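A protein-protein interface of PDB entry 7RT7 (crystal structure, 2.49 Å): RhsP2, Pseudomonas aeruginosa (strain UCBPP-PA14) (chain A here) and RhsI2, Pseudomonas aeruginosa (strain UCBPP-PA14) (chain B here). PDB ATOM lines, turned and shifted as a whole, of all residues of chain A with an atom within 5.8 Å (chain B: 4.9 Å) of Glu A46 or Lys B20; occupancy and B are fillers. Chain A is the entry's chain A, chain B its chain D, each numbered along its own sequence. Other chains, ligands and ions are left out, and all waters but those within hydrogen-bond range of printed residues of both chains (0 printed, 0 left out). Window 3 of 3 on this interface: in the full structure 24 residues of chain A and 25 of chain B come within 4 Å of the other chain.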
ATOM      1  N   HIS A  37      -1.504  14.538 -26.765  1.00  0.00           N
ATOM      2  CA  HIS A  37      -2.522  13.746 -27.445  1.00  0.00           C
ATOM      3  C   HIS A  37      -2.029  12.337 -27.739  1.00  0.00           C
ATOM      4  O   HIS A  37      -2.822  11.388 -27.734  1.00  0.00           O
ATOM      5  CB  HIS A  37      -2.946  14.440 -28.740  1.00  0.00           C
ATOM      6  CG  HIS A  37      -3.886  15.587 -28.536  1.00  0.00           C
ATOM      7  ND1 HIS A  37      -4.442  15.887 -27.311  1.00  0.00           N
ATOM      8  CD2 HIS A  37      -4.370  16.508 -29.403  1.00  0.00           C
ATOM      9  CE1 HIS A  37      -5.224  16.944 -27.432  1.00  0.00           C
ATOM     10  NE2 HIS A  37      -5.199  17.340 -28.692  1.00  0.00           N
ATOM     11  N   ILE A  40      -2.431  10.057 -24.703  1.00  0.00           N
ATOM     12  CA  ILE A  40      -3.797   9.564 -24.574  1.00  0.00           C
ATOM     13  C   ILE A  40      -4.057   8.443 -25.572  1.00  0.00           C
ATOM     14  O   ILE A  40      -4.762   7.473 -25.268  1.00  0.00           O
ATOM     15  CB  ILE A  40      -4.793  10.724 -24.757  1.00  0.00           C
ATOM     16  CG1 ILE A  40      -4.566  11.800 -23.692  1.00  0.00           C
ATOM     17  CG2 ILE A  40      -6.224  10.216 -24.706  1.00  0.00           C
ATOM     18  CD1 ILE A  40      -4.980  13.186 -24.136  1.00  0.00           C
ATOM     19  N   LEU A  41      -3.496   8.556 -26.777  1.00  0.00           N
ATOM     20  CA  LEU A  41      -3.748   7.552 -27.806  1.00  0.00           C
ATOM     21  C   LEU A  41      -3.190   6.196 -27.400  1.00  0.00           C
ATOM     22  O   LEU A  41      -3.807   5.157 -27.662  1.00  0.00           O
ATOM     23  CB  LEU A  41      -3.147   8.008 -29.134  1.00  0.00           C
ATOM     24  CG  LEU A  41      -3.352   7.090 -30.342  1.00  0.00           C
ATOM     25  CD1 LEU A  41      -4.812   6.686 -30.501  1.00  0.00           C
ATOM     26  CD2 LEU A  41      -2.847   7.782 -31.600  1.00  0.00           C
ATOM     27  N   ASN A  43      -2.693   5.256 -24.195  1.00  0.00           N
ATOM     28  CA  ASN A  43      -3.239   4.845 -22.910  1.00  0.00           C
ATOM     29  C   ASN A  43      -4.761   4.813 -22.870  1.00  0.00           C
ATOM     30  O   ASN A  43      -5.324   4.114 -22.021  1.00  0.00           O
ATOM     31  CB  ASN A  43      -2.718   5.780 -21.811  1.00  0.00           C
ATOM     32  CG  ASN A  43      -1.207   5.943 -21.859  1.00  0.00           C
ATOM     33  OD1 ASN A  43      -0.495   5.061 -22.339  1.00  0.00           O
ATOM     34  ND2 ASN A  43      -0.713   7.072 -21.368  1.00  0.00           N
ATOM     35  N   ASN A  44      -5.438   5.545 -23.757  1.00  0.00           N
ATOM     36  CA  ASN A  44      -6.891   5.513 -23.836  1.00  0.00           C
ATOM     37  C   ASN A  44      -7.413   4.910 -25.133  1.00  0.00           C
ATOM     38  O   ASN A  44      -8.605   4.592 -25.209  1.00  0.00           O
ATOM     39  CB  ASN A  44      -7.467   6.931 -23.689  1.00  0.00           C
ATOM     40  CG  ASN A  44      -7.377   7.453 -22.271  1.00  0.00           C
ATOM     41  OD1 ASN A  44      -6.385   7.235 -21.578  1.00  0.00           O
ATOM     42  ND2 ASN A  44      -8.418   8.152 -21.832  1.00  0.00           N
ATOM     43  N   PHE A  45      -6.564   4.746 -26.146  1.00  0.00           N
ATOM     44  CA  PHE A  45      -6.996   4.266 -27.459  1.00  0.00           C
ATOM     45  C   PHE A  45      -8.079   5.174 -28.035  1.00  0.00           C
ATOM     46  O   PHE A  45      -9.071   4.714 -28.604  1.00  0.00           O
ATOM     47  CB  PHE A  45      -7.482   2.820 -27.390  1.00  0.00           C
ATOM     48  CG  PHE A  45      -7.147   2.011 -28.610  1.00  0.00           C
ATOM     49  CD1 PHE A  45      -5.832   1.876 -29.026  1.00  0.00           C
ATOM     50  CD2 PHE A  45      -8.143   1.386 -29.340  1.00  0.00           C
ATOM     51  CE1 PHE A  45      -5.519   1.134 -30.145  1.00  0.00           C
ATOM     52  CE2 PHE A  45      -7.835   0.641 -30.462  1.00  0.00           C
ATOM     53  CZ  PHE A  45      -6.522   0.515 -30.865  1.00  0.00           C
ATOM     54  N   GLU A  46      -7.881   6.478 -27.876  1.00  0.00           N
ATOM     55  CA  GLU A  46      -8.789   7.494 -28.379  1.00  0.00           C
ATOM     56  C   GLU A  46      -7.985   8.577 -29.077  1.00  0.00           C
ATOM     57  O   GLU A  46      -6.852   8.877 -28.686  1.00  0.00           O
ATOM     58  CB  GLU A  46      -9.607   8.133 -27.250  1.00  0.00           C
ATOM     59  CG  GLU A  46     -10.860   7.384 -26.849  1.00  0.00           C
ATOM     60  CD  GLU A  46     -11.637   8.122 -25.777  1.00  0.00           C
ATOM     61  OE1 GLU A  46     -11.083   9.081 -25.197  1.00  0.00           O
ATOM     62  OE2 GLU A  46     -12.797   7.746 -25.511  1.00  0.00           O
ATOM     63  N   VAL A  47      -8.574   9.170 -30.107  1.00  0.00           N
ATOM     64  CA  VAL A  47      -8.049  10.387 -30.716  1.00  0.00           C
ATOM     65  C   VAL A  47      -8.605  11.567 -29.925  1.00  0.00           C
ATOM     66  O   VAL A  47      -9.829  11.763 -29.913  1.00  0.00           O
ATOM     67  CB  VAL A  47      -8.425  10.495 -32.197  1.00  0.00           C
ATOM     68  CG1 VAL A  47      -8.017  11.857 -32.738  1.00  0.00           C
ATOM     69  CG2 VAL A  47      -7.757   9.388 -32.988  1.00  0.00           C
ATOM     70  N   PRO A  48      -7.767  12.355 -29.248  1.00  0.00           N
ATOM     71  CA  PRO A  48      -8.298  13.445 -28.432  1.00  0.00           C
ATOM     72  C   PRO A  48      -8.825  14.571 -29.302  1.00  0.00           C
ATOM     73  O   PRO A  48      -8.351  14.776 -30.433  1.00  0.00           O
ATOM     74  CB  PRO A  48      -7.082  13.898 -27.604  1.00  0.00           C
ATOM     75  CG  PRO A  48      -6.035  12.850 -27.805  1.00  0.00           C
ATOM     76  CD  PRO A  48      -6.306  12.229 -29.123  1.00  0.00           C
ATOM     77  N   ASN A 145     -13.534   6.775 -32.952  1.00  0.00           N
ATOM     78  CA  ASN A 145     -12.882   6.125 -31.820  1.00  0.00           C
ATOM     79  C   ASN A 145     -13.499   4.764 -31.524  1.00  0.00           C
ATOM     80  O   ASN A 145     -12.791   3.834 -31.123  1.00  0.00           O
ATOM     81  CB  ASN A 145     -12.953   7.023 -30.587  1.00  0.00           C
ATOM     82  CG  ASN A 145     -11.960   8.169 -30.642  1.00  0.00           C
ATOM     83  OD1 ASN A 145     -10.883   8.047 -31.225  1.00  0.00           O
ATOM     84  ND2 ASN A 145     -12.321   9.293 -30.032  1.00  0.00           N
ATOM     85  N   LEU A 148     -12.013   2.495 -34.041  1.00  0.00           N
ATOM     86  CA  LEU A 148     -10.558   2.452 -34.085  1.00  0.00           C
ATOM     87  C   LEU A 148     -10.063   1.053 -33.750  1.00  0.00           C
ATOM     88  O   LEU A 148     -10.478   0.453 -32.754  1.00  0.00           O
ATOM     89  CB  LEU A 148      -9.963   3.471 -33.115  1.00  0.00           C
ATOM     90  CG  LEU A 148      -8.452   3.673 -33.248  1.00  0.00           C
ATOM     91  CD1 LEU A 148      -8.103   4.277 -34.600  1.00  0.00           C
ATOM     92  CD2 LEU A 148      -7.919   4.540 -32.118  1.00  0.00           C
ATOM     93  N   GLU B  16     -10.842  10.657 -15.460  1.00  0.00           N
ATOM     94  CA  GLU B  16     -11.409  10.015 -16.640  1.00  0.00           C
ATOM     95  C   GLU B  16     -10.321   9.358 -17.478  1.00  0.00           C
ATOM     96  O   GLU B  16     -10.510   8.251 -17.998  1.00  0.00           O
ATOM     97  CB  GLU B  16     -12.177  11.051 -17.462  1.00  0.00           C
ATOM     98  CG  GLU B  16     -13.089  10.466 -18.518  1.00  0.00           C
ATOM     99  CD  GLU B  16     -14.374   9.915 -17.933  1.00  0.00           C
ATOM    100  OE1 GLU B  16     -14.503   9.894 -16.690  1.00  0.00           O
ATOM    101  OE2 GLU B  16     -15.256   9.503 -18.715  1.00  0.00           O
ATOM    102  N   TYR B  17      -9.179  10.031 -17.623  1.00  0.00           N
ATOM    103  CA  TYR B  17      -8.025   9.428 -18.285  1.00  0.00           C
ATOM    104  C   TYR B  17      -7.582   8.164 -17.561  1.00  0.00           C
ATOM    105  O   TYR B  17      -7.212   7.170 -18.197  1.00  0.00           O
ATOM    106  CB  TYR B  17      -6.898  10.463 -18.348  1.00  0.00           C
ATOM    107  CG  TYR B  17      -5.531   9.948 -18.740  1.00  0.00           C
ATOM    108  CD1 TYR B  17      -5.251   9.580 -20.047  1.00  0.00           C
ATOM    109  CD2 TYR B  17      -4.508   9.869 -17.803  1.00  0.00           C
ATOM    110  CE1 TYR B  17      -3.996   9.126 -20.407  1.00  0.00           C
ATOM    111  CE2 TYR B  17      -3.252   9.416 -18.154  1.00  0.00           C
ATOM    112  CZ  TYR B  17      -3.001   9.047 -19.456  1.00  0.00           C
ATOM    113  OH  TYR B  17      -1.751   8.598 -19.807  1.00  0.00           O
ATOM    114  N   ILE B  18      -7.636   8.176 -16.228  1.00  0.00           N
ATOM    115  CA  ILE B  18      -7.186   7.027 -15.449  1.00  0.00           C
ATOM    116  C   ILE B  18      -8.160   5.862 -15.598  1.00  0.00           C
ATOM    117  O   ILE B  18      -7.748   4.716 -15.814  1.00  0.00           O
ATOM    118  CB  ILE B  18      -7.007   7.422 -13.972  1.00  0.00           C
ATOM    119  CG1 ILE B  18      -5.873   8.443 -13.823  1.00  0.00           C
ATOM    120  CG2 ILE B  18      -6.752   6.188 -13.116  1.00  0.00           C
ATOM    121  CD1 ILE B  18      -4.521   7.955 -14.308  1.00  0.00           C
ATOM    122  N   ARG B  19      -9.462   6.129 -15.471  1.00  0.00           N
ATOM    123  CA  ARG B  19     -10.442   5.051 -15.556  1.00  0.00           C
ATOM    124  C   ARG B  19     -10.329   4.315 -16.886  1.00  0.00           C
ATOM    125  O   ARG B  19     -10.261   3.083 -16.926  1.00  0.00           O
ATOM    126  CB  ARG B  19     -11.859   5.600 -15.370  1.00  0.00           C
ATOM    127  CG  ARG B  19     -12.951   4.541 -15.531  1.00  0.00           C
ATOM    128  CD  ARG B  19     -14.347   5.145 -15.482  1.00  0.00           C
ATOM    129  NE  ARG B  19     -14.587   6.057 -16.594  1.00  0.00           N
ATOM    130  CZ  ARG B  19     -14.968   5.682 -17.808  1.00  0.00           C
ATOM    131  NH1 ARG B  19     -15.172   4.410 -18.109  1.00  0.00           N
ATOM    132  NH2 ARG B  19     -15.146   6.609 -18.745  1.00  0.00           N
ATOM    133  N   LYS B  20     -10.310   5.064 -17.990  1.00  0.00           N
ATOM    134  CA  LYS B  20     -10.261   4.441 -19.307  1.00  0.00           C
ATOM    135  C   LYS B  20      -8.969   3.663 -19.510  1.00  0.00           C
ATOM    136  O   LYS B  20      -8.957   2.658 -20.230  1.00  0.00           O
ATOM    137  CB  LYS B  20     -10.428   5.509 -20.385  1.00  0.00           C
ATOM    138  CG  LYS B  20     -11.806   6.149 -20.378  1.00  0.00           C
ATOM    139  CD  LYS B  20     -11.850   7.419 -21.211  1.00  0.00           C
ATOM    140  CE  LYS B  20     -11.921   7.113 -22.697  1.00  0.00           C
ATOM    141  NZ  LYS B  20     -13.102   6.277 -23.058  1.00  0.00           N
ATOM    142  N   ALA B  21      -7.875   4.104 -18.886  1.00  0.00           N
ATOM    143  CA  ALA B  21      -6.624   3.361 -18.980  1.00  0.00           C
ATOM    144  C   ALA B  21      -6.749   2.000 -18.309  1.00  0.00           C
ATOM    145  O   ALA B  21      -6.359   0.974 -18.879  1.00  0.00           O
ATOM    146  CB  ALA B  21      -5.487   4.169 -18.352  1.00  0.00           C
ATOM    147  N   HIS B  22      -7.296   1.972 -17.091  1.00  0.00           N
ATOM    148  CA  HIS B  22      -7.463   0.708 -16.383  1.00  0.00           C
ATOM    149  C   HIS B  22      -8.462  -0.195 -17.093  1.00  0.00           C
ATOM    150  O   HIS B  22      -8.252  -1.411 -17.186  1.00  0.00           O
ATOM    151  CB  HIS B  22      -7.908   0.976 -14.946  1.00  0.00           C
ATOM    152  CG  HIS B  22      -6.898   1.726 -14.135  1.00  0.00           C
ATOM    153  ND1 HIS B  22      -7.097   2.056 -12.811  1.00  0.00           N
ATOM    154  CD2 HIS B  22      -5.680   2.216 -14.466  1.00  0.00           C
ATOM    155  CE1 HIS B  22      -6.043   2.711 -12.361  1.00  0.00           C
ATOM    156  NE2 HIS B  22      -5.168   2.821 -13.344  1.00  0.00           N
ATOM    157  N   GLU B  23      -9.554   0.378 -17.602  1.00  0.00           N
ATOM    158  CA  GLU B  23     -10.540  -0.427 -18.312  1.00  0.00           C
ATOM    159  C   GLU B  23      -9.963  -0.976 -19.610  1.00  0.00           C
ATOM    160  O   GLU B  23     -10.268  -2.107 -20.001  1.00  0.00           O
ATOM    161  CB  GLU B  23     -11.797   0.399 -18.583  1.00  0.00           C
ATOM    162  CG  GLU B  23     -12.877   0.207 -17.530  1.00  0.00           C
ATOM    163  CD  GLU B  23     -13.783   1.414 -17.383  1.00  0.00           C
ATOM    164  OE1 GLU B  23     -13.784   2.275 -18.288  1.00  0.00           O
ATOM    165  OE2 GLU B  23     -14.499   1.499 -16.362  1.00  0.00           O
ATOM    166  N   LEU B  24      -9.119  -0.194 -20.288  1.00  0.00           N
ATOM    167  CA  LEU B  24      -8.467  -0.693 -21.492  1.00  0.00           C
ATOM    168  C   LEU B  24      -7.428  -1.756 -21.162  1.00  0.00           C
ATOM    169  O   LEU B  24      -7.235  -2.700 -21.937  1.00  0.00           O
ATOM    170  CB  LEU B  24      -7.815   0.458 -22.254  1.00  0.00           C
ATOM    171  CG  LEU B  24      -7.298   0.120 -23.652  1.00  0.00           C
ATOM    172  CD1 LEU B  24      -8.405  -0.456 -24.525  1.00  0.00           C
ATOM    173  CD2 LEU B  24      -6.696   1.357 -24.287  1.00  0.00           C
ATOM    174  N   THR B  25      -6.748  -1.616 -20.022  1.00  0.00           N
ATOM    175  CA  THR B  25      -5.762  -2.613 -19.617  1.00  0.00           C
ATOM    176  C   THR B  25      -6.436  -3.919 -19.217  1.00  0.00           C
ATOM    177  O   THR B  25      -5.983  -5.002 -19.603  1.00  0.00           O
ATOM    178  CB  THR B  25      -4.921  -2.073 -18.458  1.00  0.00           C
ATOM    179  OG1 THR B  25      -4.022  -1.066 -18.938  1.00  0.00           O
ATOM    180  CG2 THR B  25      -4.128  -3.192 -17.798  1.00  0.00           C
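Ala B21 touches Asn A43 (CA to O, 3.4 Å). Leu B24 touches Asn A43. CD of Lys B20 touches ND2 of Asn A44, at 3.6 Å. Asn A44 touches Leu B24. CD2 of Leu B24 touches CB of Phe A45 (3.5 Å).
Glu A46 touches just one residue of chain B: Lys B20. Lys B20 touches just these residues of chain A: Asn A44 and Glu A46. Of the printed residues of chain B, Asn A44 touches Tyr B17, Lys B20 and Leu B24. Of the printed residues of chain A, Tyr B17 touches Asn A43 and Asn A44. The nearest printed residue of chain B that does not touch Asn A44 is Glu B16 (4.4 Å).
Of the 10 printed residues of chain B, 4 touch a printed residue of chain A. Printed residues of chain A that touch a printed residue of chain B: Asn A43, Asn A44, Phe A45 and Glu A46. Along chain A the printed residues that touch a printed residue of chain B span positions 43 to 46. Among the printed residues, Asp or Glu carboxylates within 4 Å of a Lys or Arg side-chain nitrogen of the other chain: Glu A46 with Lys B20.
OD1 of Asn A44 sits close to O of Tyr B17, 3.5 Å away. The side-chain hydroxyl of Tyr B17 lies within hydrogen-bond range of the side-chain amide nitrogen of Asn A43 (2.4 Å). The side-chain carboxylate (OE2) of Glu A46 is in salt-bridge range of the side-chain amino group (NZ) of Lys B20.
O of Ala B21 lies within hydrogen-bond range of OG1 of Thr B25, at 3.1 Å. The backbone carbonyl oxygen of Ile A40 is in hydrogen-bond range of the backbone NH of Phe A45, at 3.4 Å.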
